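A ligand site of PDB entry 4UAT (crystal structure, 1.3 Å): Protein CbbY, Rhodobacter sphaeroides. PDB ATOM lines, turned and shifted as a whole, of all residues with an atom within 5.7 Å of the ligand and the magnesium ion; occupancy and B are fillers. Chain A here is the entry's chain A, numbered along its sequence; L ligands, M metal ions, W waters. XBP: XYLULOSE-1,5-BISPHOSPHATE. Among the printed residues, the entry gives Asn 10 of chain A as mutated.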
ATOM      1  N   ASP A   8       5.475   0.451  26.920  1.00  0.00           N
ATOM      2  CA  ASP A   8       4.929  -0.843  26.589  1.00  0.00           C
ATOM      3  C   ASP A   8       4.053  -1.334  27.736  1.00  0.00           C
ATOM      4  O   ASP A   8       4.160  -0.865  28.879  1.00  0.00           O
ATOM      5  CB  ASP A   8       6.086  -1.786  26.346  1.00  0.00           C
ATOM      6  CG  ASP A   8       5.662  -3.148  25.969  1.00  0.00           C
ATOM      7  OD1 ASP A   8       4.873  -3.249  24.998  1.00  0.00           O
ATOM      8  OD2 ASP A   8       6.061  -4.122  26.639  1.00  0.00           O
ATOM      9  N   VAL A   9       3.233  -2.350  27.495  1.00  0.00           N
ATOM     10  CA  VAL A   9       2.393  -2.918  28.536  1.00  0.00           C
ATOM     11  C   VAL A   9       2.929  -4.286  28.999  1.00  0.00           C
ATOM     12  O   VAL A   9       3.444  -4.383  30.131  1.00  0.00           O
ATOM     13  CB  VAL A   9       0.927  -2.973  28.131  1.00  0.00           C
ATOM     14  CG1 VAL A   9       0.077  -3.718  29.197  1.00  0.00           C
ATOM     15  CG2 VAL A   9       0.403  -1.554  27.933  1.00  0.00           C
ATOM     16  N   ASN A  10       2.809  -5.336  28.182  1.00  0.00           N
ATOM     17  CA  ASN A  10       3.119  -6.655  28.655  1.00  0.00           C
ATOM     18  C   ASN A  10       4.622  -6.848  28.821  1.00  0.00           C
ATOM     19  O   ASN A  10       5.405  -6.650  27.898  1.00  0.00           O
ATOM     20  CB  ASN A  10       2.520  -7.711  27.702  1.00  0.00           C
ATOM     21  CG  ASN A  10       1.026  -7.619  27.646  1.00  0.00           C
ATOM     22  OD1 ASN A  10       0.372  -7.809  28.733  1.00  0.00           O
ATOM     23  ND2 ASN A  10       0.424  -7.375  26.509  1.00  0.00           N
ATOM     24  N   GLY A  11       4.964  -7.281  30.028  1.00  0.00           N
ATOM     25  CA  GLY A  11       6.332  -7.421  30.440  1.00  0.00           C
ATOM     26  C   GLY A  11       7.035  -6.157  30.888  1.00  0.00           C
ATOM     27  O   GLY A  11       8.147  -6.221  31.379  1.00  0.00           O
ATOM     28  N   THR A  12       6.354  -5.027  30.767  1.00  0.00           N
ATOM     29  CA  THR A  12       6.915  -3.705  31.054  1.00  0.00           C
ATOM     30  C   THR A  12       6.215  -3.098  32.272  1.00  0.00           C
ATOM     31  O   THR A  12       6.818  -2.900  33.288  1.00  0.00           O
ATOM     32  CB  THR A  12       6.928  -2.825  29.787  1.00  0.00           C
ATOM     33  OG1 THR A  12       7.748  -3.424  28.775  1.00  0.00           O
ATOM     34  CG2 THR A  12       7.477  -1.423  30.081  1.00  0.00           C
ATOM     35  N   GLU A  17       2.717 -12.294  30.956  1.00  0.00           N
ATOM     36  CA  GLU A  17       2.595 -13.280  29.917  1.00  0.00           C
ATOM     37  C   GLU A  17       2.173 -14.647  30.372  1.00  0.00           C
ATOM     38  O   GLU A  17       1.473 -15.320  29.628  1.00  0.00           O
ATOM     39  CB  GLU A  17       3.801 -13.335  29.004  1.00  0.00           C
ATOM     40  CG  GLU A  17       3.870 -12.190  27.985  1.00  0.00           C
ATOM     41  CD  GLU A  17       2.728 -12.182  26.960  1.00  0.00           C
ATOM     42  OE1 GLU A  17       1.953 -13.163  26.896  1.00  0.00           O
ATOM     43  OE2 GLU A  17       2.705 -11.192  26.165  1.00  0.00           O
ATOM     44  N   HIS A  20      -1.499 -14.296  30.347  1.00  0.00           N
ATOM     45  CA  HIS A  20      -1.970 -14.458  28.954  1.00  0.00           C
ATOM     46  C   HIS A  20      -1.997 -15.931  28.574  1.00  0.00           C
ATOM     47  O   HIS A  20      -2.988 -16.380  27.982  1.00  0.00           O
ATOM     48  CB  HIS A  20      -1.158 -13.666  27.966  1.00  0.00           C
ATOM     49  CG  HIS A  20      -1.401 -12.188  28.037  1.00  0.00           C
ATOM     50  ND1 HIS A  20      -2.560 -11.608  27.558  1.00  0.00           N
ATOM     51  CD2 HIS A  20      -0.610 -11.171  28.485  1.00  0.00           C
ATOM     52  CE1 HIS A  20      -2.461 -10.294  27.705  1.00  0.00           C
ATOM     53  NE2 HIS A  20      -1.308 -10.003  28.286  1.00  0.00           N
ATOM     54  N   PHE A  24      -5.229 -18.034  27.302  1.00  0.00           N
ATOM     55  CA  PHE A  24      -5.289 -18.798  26.048  1.00  0.00           C
ATOM     56  C   PHE A  24      -5.719 -20.237  26.314  1.00  0.00           C
ATOM     57  O   PHE A  24      -6.643 -20.747  25.741  1.00  0.00           O
ATOM     58  CB  PHE A  24      -4.000 -18.728  25.232  1.00  0.00           C
ATOM     59  CG  PHE A  24      -3.741 -17.447  24.511  1.00  0.00           C
ATOM     60  CD1 PHE A  24      -4.425 -17.091  23.356  1.00  0.00           C
ATOM     61  CD2 PHE A  24      -2.712 -16.620  24.878  1.00  0.00           C
ATOM     62  CE1 PHE A  24      -4.124 -15.953  22.642  1.00  0.00           C
ATOM     63  CE2 PHE A  24      -2.420 -15.475  24.172  1.00  0.00           C
ATOM     64  CZ  PHE A  24      -3.121 -15.138  23.052  1.00  0.00           C
ATOM     65  N   TYR A  42       4.992 -21.445  23.873  1.00  0.00           N
ATOM     66  CA  TYR A  42       4.592 -20.031  24.022  1.00  0.00           C
ATOM     67  C   TYR A  42       5.776 -19.079  23.837  1.00  0.00           C
ATOM     68  O   TYR A  42       5.614 -18.020  23.246  1.00  0.00           O
ATOM     69  CB  TYR A  42       3.890 -19.817  25.367  1.00  0.00           C
ATOM     70  CG  TYR A  42       3.076 -18.542  25.430  1.00  0.00           C
ATOM     71  CD1 TYR A  42       1.997 -18.366  24.554  1.00  0.00           C
ATOM     72  CD2 TYR A  42       3.295 -17.526  26.372  1.00  0.00           C
ATOM     73  CE1 TYR A  42       1.201 -17.242  24.603  1.00  0.00           C
ATOM     74  CE2 TYR A  42       2.514 -16.373  26.376  1.00  0.00           C
ATOM     75  CZ  TYR A  42       1.504 -16.210  25.495  1.00  0.00           C
ATOM     76  OH  TYR A  42       0.754 -15.067  25.456  1.00  0.00           O
ATOM     77  N   LEU A  46       5.475 -16.114  21.135  1.00  0.00           N
ATOM     78  CA  LEU A  46       5.571 -14.732  21.575  1.00  0.00           C
ATOM     79  C   LEU A  46       6.356 -13.851  20.633  1.00  0.00           C
ATOM     80  O   LEU A  46       6.274 -12.609  20.758  1.00  0.00           O
ATOM     81  CB  LEU A  46       6.162 -14.628  22.988  1.00  0.00           C
ATOM     82  CG  LEU A  46       5.201 -14.907  24.130  1.00  0.00           C
ATOM     83  CD1 LEU A  46       5.908 -15.109  25.449  1.00  0.00           C
ATOM     84  CD2 LEU A  46       4.153 -13.790  24.269  1.00  0.00           C
ATOM     85  N   THR A  48       5.657 -13.476  17.614  1.00  0.00           N
ATOM     86  CA  THR A  48       4.586 -12.843  16.841  1.00  0.00           C
ATOM     87  C   THR A  48       3.681 -12.076  17.809  1.00  0.00           C
ATOM     88  O   THR A  48       3.083 -12.694  18.683  1.00  0.00           O
ATOM     89  CB  THR A  48       3.762 -13.910  16.141  1.00  0.00           C
ATOM     90  OG1 THR A  48       4.608 -14.634  15.242  1.00  0.00           O
ATOM     91  CG2 THR A  48       2.606 -13.353  15.431  1.00  0.00           C
ATOM     92  N   THR A  49       3.638 -10.746  17.680  1.00  0.00           N
ATOM     93  CA  THR A  49       2.833  -9.961  18.540  1.00  0.00           C
ATOM     94  C   THR A  49       1.384  -9.876  18.075  1.00  0.00           C
ATOM     95  O   THR A  49       1.052 -10.001  16.910  1.00  0.00           O
ATOM     96  CB  THR A  49       3.382  -8.563  18.735  1.00  0.00           C
ATOM     97  OG1 THR A  49       3.198  -7.818  17.518  1.00  0.00           O
ATOM     98  CG2 THR A  49       4.848  -8.588  19.183  1.00  0.00           C
ATOM     99  N   GLY A  50       0.495  -9.739  19.079  1.00  0.00           N
ATOM    100  CA  GLY A  50      -0.942  -9.727  18.882  1.00  0.00           C
ATOM    101  C   GLY A  50      -1.482 -11.120  18.998  1.00  0.00           C
ATOM    102  O   GLY A  50      -1.014 -12.064  18.356  1.00  0.00           O
ATOM    103  N   GLY A  51      -2.524 -11.255  19.843  1.00  0.00           N
ATOM    104  CA  GLY A  51      -3.027 -12.622  20.110  1.00  0.00           C
ATOM    105  C   GLY A  51      -3.721 -13.239  18.907  1.00  0.00           C
ATOM    106  O   GLY A  51      -3.700 -14.449  18.717  1.00  0.00           O
ATOM    107  N   LYS A  52      -4.443 -12.419  18.111  1.00  0.00           N
ATOM    108  CA  LYS A  52      -5.058 -12.955  16.899  1.00  0.00           C
ATOM    109  C   LYS A  52      -4.000 -13.472  15.943  1.00  0.00           C
ATOM    110  O   LYS A  52      -4.124 -14.577  15.346  1.00  0.00           O
ATOM    111  CB  LYS A  52      -5.949 -11.915  16.217  1.00  0.00           C
ATOM    112  CG  LYS A  52      -7.150 -11.557  17.056  1.00  0.00           C
ATOM    113  CD  LYS A  52      -8.166 -10.644  16.303  1.00  0.00           C
ATOM    114  CE  LYS A  52      -7.615  -9.291  15.967  1.00  0.00           C
ATOM    115  NZ  LYS A  52      -7.185  -8.490  17.097  1.00  0.00           N
ATOM    116  N   ARG A  54      -1.005 -14.382  16.718  1.00  0.00           N
ATOM    117  CA  ARG A  54      -0.349 -15.518  17.309  1.00  0.00           C
ATOM    118  C   ARG A  54      -1.174 -16.791  17.050  1.00  0.00           C
ATOM    119  O   ARG A  54      -0.636 -17.826  16.697  1.00  0.00           O
ATOM    120  CB  ARG A  54      -0.129 -15.282  18.826  1.00  0.00           C
ATOM    121  CG  ARG A  54       0.685 -16.352  19.515  1.00  0.00           C
ATOM    122  CD  ARG A  54       1.016 -15.970  20.968  1.00  0.00           C
ATOM    123  NE  ARG A  54       1.772 -14.778  20.957  1.00  0.00           N
ATOM    124  CZ  ARG A  54       1.492 -13.692  21.633  1.00  0.00           C
ATOM    125  NH1 ARG A  54       0.728 -13.735  22.729  1.00  0.00           N
ATOM    126  NH2 ARG A  54       2.028 -12.551  21.281  1.00  0.00           N
ATOM    127  N   HIS A  75     -10.311 -15.150  20.138  1.00  0.00           N
ATOM    128  CA  HIS A  75      -9.518 -14.157  20.825  1.00  0.00           C
ATOM    129  C   HIS A  75     -10.406 -13.290  21.794  1.00  0.00           C
ATOM    130  O   HIS A  75      -9.933 -12.883  22.840  1.00  0.00           O
ATOM    131  CB  HIS A  75      -8.719 -13.322  19.849  1.00  0.00           C
ATOM    132  CG  HIS A  75      -7.758 -12.439  20.568  1.00  0.00           C
ATOM    133  ND1 HIS A  75      -7.938 -11.120  20.762  1.00  0.00           N
ATOM    134  CD2 HIS A  75      -6.584 -12.759  21.200  1.00  0.00           C
ATOM    135  CE1 HIS A  75      -6.941 -10.636  21.471  1.00  0.00           C
ATOM    136  NE2 HIS A  75      -6.121 -11.605  21.739  1.00  0.00           N
ATOM    137  N   LYS A  78     -10.792 -15.185  24.889  1.00  0.00           N
ATOM    138  CA  LYS A  78      -9.560 -15.135  25.633  1.00  0.00           C
ATOM    139  C   LYS A  78      -9.393 -13.791  26.360  1.00  0.00           C
ATOM    140  O   LYS A  78      -8.882 -13.769  27.475  1.00  0.00           O
ATOM    141  CB  LYS A  78      -8.396 -15.435  24.699  1.00  0.00           C
ATOM    142  CG  LYS A  78      -7.016 -15.257  25.338  1.00  0.00           C
ATOM    143  CD  LYS A  78      -6.403 -13.899  25.138  1.00  0.00           C
ATOM    144  CE  LYS A  78      -5.154 -13.666  25.937  1.00  0.00           C
ATOM    145  NZ  LYS A  78      -4.610 -12.295  25.743  1.00  0.00           N
ATOM    146  N   THR A  79      -9.761 -12.700  25.664  1.00  0.00           N
ATOM    147  CA  THR A  79      -9.650 -11.389  26.286  1.00  0.00           C
ATOM    148  C   THR A  79     -10.568 -11.265  27.495  1.00  0.00           C
ATOM    149  O   THR A  79     -10.177 -10.742  28.545  1.00  0.00           O
ATOM    150  CB  THR A  79      -9.914 -10.310  25.260  1.00  0.00           C
ATOM    151  OG1 THR A  79      -8.945 -10.373  24.203  1.00  0.00           O
ATOM    152  CG2 THR A  79      -9.890  -8.919  25.846  1.00  0.00           C
ATOM    153  N   ALA A 114       1.960   2.348  24.463  1.00  0.00           N
ATOM    154  CA  ALA A 114       2.154   1.910  23.079  1.00  0.00           C
ATOM    155  C   ALA A 114       2.357   0.405  23.097  1.00  0.00           C
ATOM    156  O   ALA A 114       3.412  -0.077  23.492  1.00  0.00           O
ATOM    157  CB  ALA A 114       3.331   2.596  22.426  1.00  0.00           C
ATOM    158  N   THR A 115       1.286  -0.337  22.757  1.00  0.00           N
ATOM    159  CA  THR A 115       1.187  -1.763  23.011  1.00  0.00           C
ATOM    160  C   THR A 115       0.594  -2.465  21.827  1.00  0.00           C
ATOM    161  O   THR A 115      -0.275  -1.966  21.163  1.00  0.00           O
ATOM    162  CB  THR A 115       0.401  -2.062  24.322  1.00  0.00           C
ATOM    163  OG1 THR A 115       0.334  -3.483  24.535  1.00  0.00           O
ATOM    164  CG2 THR A 115      -0.970  -1.530  24.284  1.00  0.00           C
ATOM    165  N   THR A 116       0.976  -3.751  21.701  1.00  0.00           N
ATOM    166  CA  THR A 116       0.319  -4.681  20.796  1.00  0.00           C
ATOM    167  C   THR A 116      -0.968  -5.261  21.363  1.00  0.00           C
ATOM    168  O   THR A 116      -1.731  -5.872  20.592  1.00  0.00           O
ATOM    169  CB  THR A 116       1.270  -5.801  20.375  1.00  0.00           C
ATOM    170  OG1 THR A 116       1.524  -6.666  21.460  1.00  0.00           O
ATOM    171  CG2 THR A 116       2.541  -5.226  19.767  1.00  0.00           C
ATOM    172  N   THR A 117      -1.198  -5.135  22.664  1.00  0.00           N
ATOM    173  CA  THR A 117      -2.226  -5.857  23.353  1.00  0.00           C
ATOM    174  C   THR A 117      -3.605  -5.207  23.153  1.00  0.00           C
ATOM    175  O   THR A 117      -3.721  -4.036  22.827  1.00  0.00           O
ATOM    176  CB  THR A 117      -1.884  -5.934  24.853  1.00  0.00           C
ATOM    177  OG1 THR A 117      -2.377  -7.154  25.452  1.00  0.00           O
ATOM    178  CG2 THR A 117      -2.370  -4.792  25.724  1.00  0.00           C
ATOM    179  N   SER A 118      -4.623  -5.992  23.398  1.00  0.00           N
ATOM    180  CA  SER A 118      -6.033  -5.540  23.266  1.00  0.00           C
ATOM    181  C   SER A 118      -6.329  -4.426  24.268  1.00  0.00           C
ATOM    182  O   SER A 118      -5.916  -4.518  25.424  1.00  0.00           O
ATOM    183  CB  SER A 118      -6.956  -6.683  23.488  1.00  0.00           C
ATOM    184  OG  SER A 118      -6.642  -7.740  22.601  1.00  0.00           O
ATOM    185  N   ASN A 121      -7.374  -5.117  27.920  1.00  0.00           N
ATOM    186  CA  ASN A 121      -6.311  -5.523  28.832  1.00  0.00           C
ATOM    187  C   ASN A 121      -5.635  -4.366  29.516  1.00  0.00           C
ATOM    188  O   ASN A 121      -5.218  -4.456  30.663  1.00  0.00           O
ATOM    189  CB  ASN A 121      -5.258  -6.334  28.094  1.00  0.00           C
ATOM    190  CG  ASN A 121      -5.790  -7.588  27.392  1.00  0.00           C
ATOM    191  OD1 ASN A 121      -6.851  -8.094  27.714  1.00  0.00           O
ATOM    192  ND2 ASN A 121      -4.989  -8.067  26.443  1.00  0.00           N
ATOM    193  N   LYS A 150       1.640  -4.586  13.670  1.00  0.00           N
ATOM    194  CA  LYS A 150       2.091  -4.595  15.019  1.00  0.00           C
ATOM    195  C   LYS A 150       3.604  -4.671  15.173  1.00  0.00           C
ATOM    196  O   LYS A 150       4.332  -4.880  14.211  1.00  0.00           O
ATOM    197  CB  LYS A 150       1.392  -5.719  15.830  1.00  0.00           C
ATOM    198  CG  LYS A 150      -0.089  -5.519  16.003  1.00  0.00           C
ATOM    199  CD  LYS A 150      -0.765  -6.596  16.777  1.00  0.00           C
ATOM    200  CE  LYS A 150      -2.195  -6.352  17.153  1.00  0.00           C
ATOM    201  NZ  LYS A 150      -3.104  -6.384  15.989  1.00  0.00           N
ATOM    202  N   LYS A 151       4.099  -4.389  16.341  1.00  0.00           N
ATOM    203  CA  LYS A 151       5.528  -4.481  16.622  1.00  0.00           C
ATOM    204  C   LYS A 151       6.055  -5.794  16.060  1.00  0.00           C
ATOM    205  O   LYS A 151       5.442  -6.827  16.264  1.00  0.00           O
ATOM    206  CB  LYS A 151       5.774  -4.376  18.131  1.00  0.00           C
ATOM    207  CG  LYS A 151       5.235  -3.105  18.802  1.00  0.00           C
ATOM    208  CD  LYS A 151       5.609  -3.037  20.282  1.00  0.00           C
ATOM    209  CE  LYS A 151       4.789  -2.056  21.110  1.00  0.00           C
ATOM    210  NZ  LYS A 151       5.028  -2.205  22.546  1.00  0.00           N
ATOM    211  N   GLU A 175      10.511  -0.653  27.353  1.00  0.00           N
ATOM    212  CA  GLU A 175      10.150  -1.926  26.698  1.00  0.00           C
ATOM    213  C   GLU A 175      10.764  -3.074  27.412  1.00  0.00           C
ATOM    214  O   GLU A 175      11.704  -2.940  28.209  1.00  0.00           O
ATOM    215  CB  GLU A 175      10.703  -1.880  25.241  1.00  0.00           C
ATOM    216  CG  GLU A 175       9.718  -1.226  24.277  1.00  0.00           C
ATOM    217  CD  GLU A 175       8.537  -2.083  23.950  1.00  0.00           C
ATOM    218  OE1 GLU A 175       8.510  -3.246  24.426  1.00  0.00           O
ATOM    219  OE2 GLU A 175       7.677  -1.651  23.138  1.00  0.00           O
ATOM    220  N   ASP A 176      10.302  -4.271  27.064  1.00  0.00           N
ATOM    221  CA  ASP A 176      10.807  -5.524  27.618  1.00  0.00           C
ATOM    222  C   ASP A 176      11.294  -6.531  26.570  1.00  0.00           C
ATOM    223  O   ASP A 176      11.935  -7.499  26.960  1.00  0.00           O
ATOM    224  CB  ASP A 176       9.712  -6.259  28.452  1.00  0.00           C
ATOM    225  CG  ASP A 176       8.608  -6.817  27.534  1.00  0.00           C
ATOM    226  OD1 ASP A 176       8.013  -6.003  26.823  1.00  0.00           O
ATOM    227  OD2 ASP A 176       8.375  -8.044  27.607  1.00  0.00           O
ATOM    228  N   SER A 177      10.953  -6.308  25.288  1.00  0.00           N
ATOM    229  CA  SER A 177      11.128  -7.336  24.281  1.00  0.00           C
ATOM    230  C   SER A 177      11.861  -6.800  23.047  1.00  0.00           C
ATOM    231  O   SER A 177      11.859  -5.590  22.840  1.00  0.00           O
ATOM    232  CB  SER A 177       9.780  -7.911  23.816  1.00  0.00           C
ATOM    233  OG  SER A 177       9.047  -7.001  23.007  1.00  0.00           O
HETATM  234  C1  XBP L   1       2.753  -8.311  23.772  1.00  0.00           C
HETATM  235  C2  XBP L   1       1.919  -9.111  22.844  1.00  0.00           C
HETATM  236  C3  XBP L   1       0.448  -9.289  23.021  1.00  0.00           C
HETATM  237  C4  XBP L   1       0.226 -10.190  24.241  1.00  0.00           C
HETATM  238  C5  XBP L   1      -1.199 -10.756  24.347  1.00  0.00           C
HETATM  239  O1  XBP L   1       2.077  -7.044  24.341  1.00  0.00           O
HETATM  240  O2  XBP L   1       2.451  -9.688  21.867  1.00  0.00           O
HETATM  241  O3  XBP L   1      -0.130  -9.842  21.844  1.00  0.00           O
HETATM  242  O4  XBP L   1       1.096 -11.352  24.163  1.00  0.00           O
HETATM  243  O5  XBP L   1      -2.201  -9.749  24.282  1.00  0.00           O
HETATM  244  P1  XBP L   1       3.036  -5.614  24.504  1.00  0.00           P
HETATM  245  P2  XBP L   1      -3.404  -9.846  23.193  1.00  0.00           P
HETATM  246  O1P XBP L   1       2.236  -4.912  25.530  1.00  0.00           O
HETATM  247  O2P XBP L   1       4.293  -6.184  25.069  1.00  0.00           O
HETATM  248  O3P XBP L   1       3.160  -5.081  23.135  1.00  0.00           O
HETATM  249  O4P XBP L   1      -4.437  -8.874  23.678  1.00  0.00           O
HETATM  250  O5P XBP L   1      -3.871 -11.277  23.203  1.00  0.00           O
HETATM  251  O6P XBP L   1      -2.792  -9.436  21.879  1.00  0.00           O
HETATM  252 MG    MG M   1       6.056  -6.018  25.999  1.00  0.00          MG
HETATM  253  O   HOH W   1       6.523  -8.050  25.569  1.00  0.00           O
HETATM  254  O   HOH W   2      -6.292 -10.343  25.004  1.00  0.00           O
HETATM  255  O   HOH W   3       5.521  -5.903  22.004  1.00  0.00           O
HETATM  256  O   HOH W   4       5.094 -10.721  22.367  1.00  0.00           O
HETATM  257  O   HOH W   5       7.070  -5.482  24.193  1.00  0.00           O
HETATM  258  O   HOH W   6       5.109 -10.334  25.385  1.00  0.00           O
HETATM  259  O   HOH W   7      -3.777  -7.661  20.138  1.00  0.00           O
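The backbone NH of Asn 10 sits at hydrogen-bond distance from an oxygen (O1P) of the ligand, 2.7 Å away. The side-chain amide nitrogen of Asn 10 is in hydrogen-bond range of an oxygen (O1) of the ligand (2.7 Å). The side-chain carboxylate (OE2) of Glu 17 lies within hydrogen-bond range of an oxygen (O4) of the ligand (2.6 Å). OG1 of Thr 115 lies within hydrogen-bond range of O1P of the ligand (2.6 Å). The backbone NH of Ser 118 is in hydrogen-bond range of an oxygen (O4P) of the ligand. O4P of the ligand is in hydrogen-bond range of OG of Ser 118, at 2.7 Å. A ring nitrogen (NE2) of His 75 lies within hydrogen-bond range of an oxygen (O5P) of the ligand (2.7 Å). The backbone NH of Gly 51 sits at hydrogen-bond distance from an oxygen (O6P) of the ligand. NH1 of Arg 54 sits at hydrogen-bond distance from O4 of the ligand (2.8 Å). O3P of the ligand is in hydrogen-bond range of N of Thr 116 (2.9 Å). An oxygen (O3P) of the ligand lies within hydrogen-bond range of the side-chain hydroxyl (OG1) of Thr 116 (2.8 Å). NZ of Lys 78 lies within salt-bridge range of O5P of the ligand, at 2.8 Å. An oxygen (O3) of the ligand lies within hydrogen-bond range of the backbone NH (N) of Gly 50, 2.8 Å away. An oxygen (O5) of the ligand lies within hydrogen-bond range of the side-chain hydroxyl (OG1) of Thr 117, 2.9 Å away. The side-chain amide nitrogen (ND2) of Asn 121 is in hydrogen-bond range of an oxygen (O4P) of the ligand. The backbone NH (N) of Val 9 lies within hydrogen-bond range of an oxygen (O1P) of the ligand (3.4 Å). The side-chain amino group of Lys 151 is in salt-bridge range of an oxygen (O3P) of the ligand (3.5 Å).
Residues that only touch the ligand: Thr 49 (3.4 Å), His 20 (3.5 Å), Leu 46 (3.9 Å), Phe 24 (3.9 Å) and Tyr 42 (3.9 Å).
Water W5 lies within hydrogen-bond range of the side-chain carboxylate (OE1) of Glu 175 (2.7 Å), the side-chain hydroxyl (OG) of Ser 177 (2.8 Å) and the side-chain carboxylate (OD1) of Asp 8 (3.2 Å). Water W7 lies within hydrogen-bond range of O6P of the ligand (2.7 Å) and O of Thr 116 (2.8 Å). Water W2 lies within hydrogen-bond range of NZ of Lys 78, O4P of the ligand, OG1 of Thr 79 and ND2 of Asn 121. Water W4 bridges the backbone carbonyl oxygen (O) of Leu 46 and an oxygen (O2) of the ligand.
The magnesium ion is bound by O2P of the ligand, OD2 of Asp 8, O of Asn 10, OD1 of Asp 176, water W1 and water W5.
The side-chain carboxylate of Asp 8 lies within salt-bridge range of the side-chain amino group of Lys 151 (2.7 Å). The side-chain amide nitrogen (ND2) of Asn 10 is in hydrogen-bond range of the side-chain hydroxyl (OG1) of Thr 117 (3.0 Å). NE2 of His 20 lies within hydrogen-bond range of OD1 of Asn 10, 2.8 Å away. OH of Tyr 42 sits at hydrogen-bond distance from OE1 of Glu 17, at 2.7 Å. The guanidinium group (NH1) of Arg 54 is in hydrogen-bond range of the side-chain hydroxyl (OH) of Tyr 42. The side-chain amino group (NZ) of Lys 78 lies within hydrogen-bond range of a ring nitrogen (ND1) of His 20, 2.8 Å away. The side-chain hydroxyl (OG1) of Thr 117 lies within hydrogen-bond range of the side-chain amide nitrogen (ND2) of Asn 121 (2.9 Å). OG1 of Thr 49 sits at hydrogen-bond distance from O of Lys 151, 2.8 Å away.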
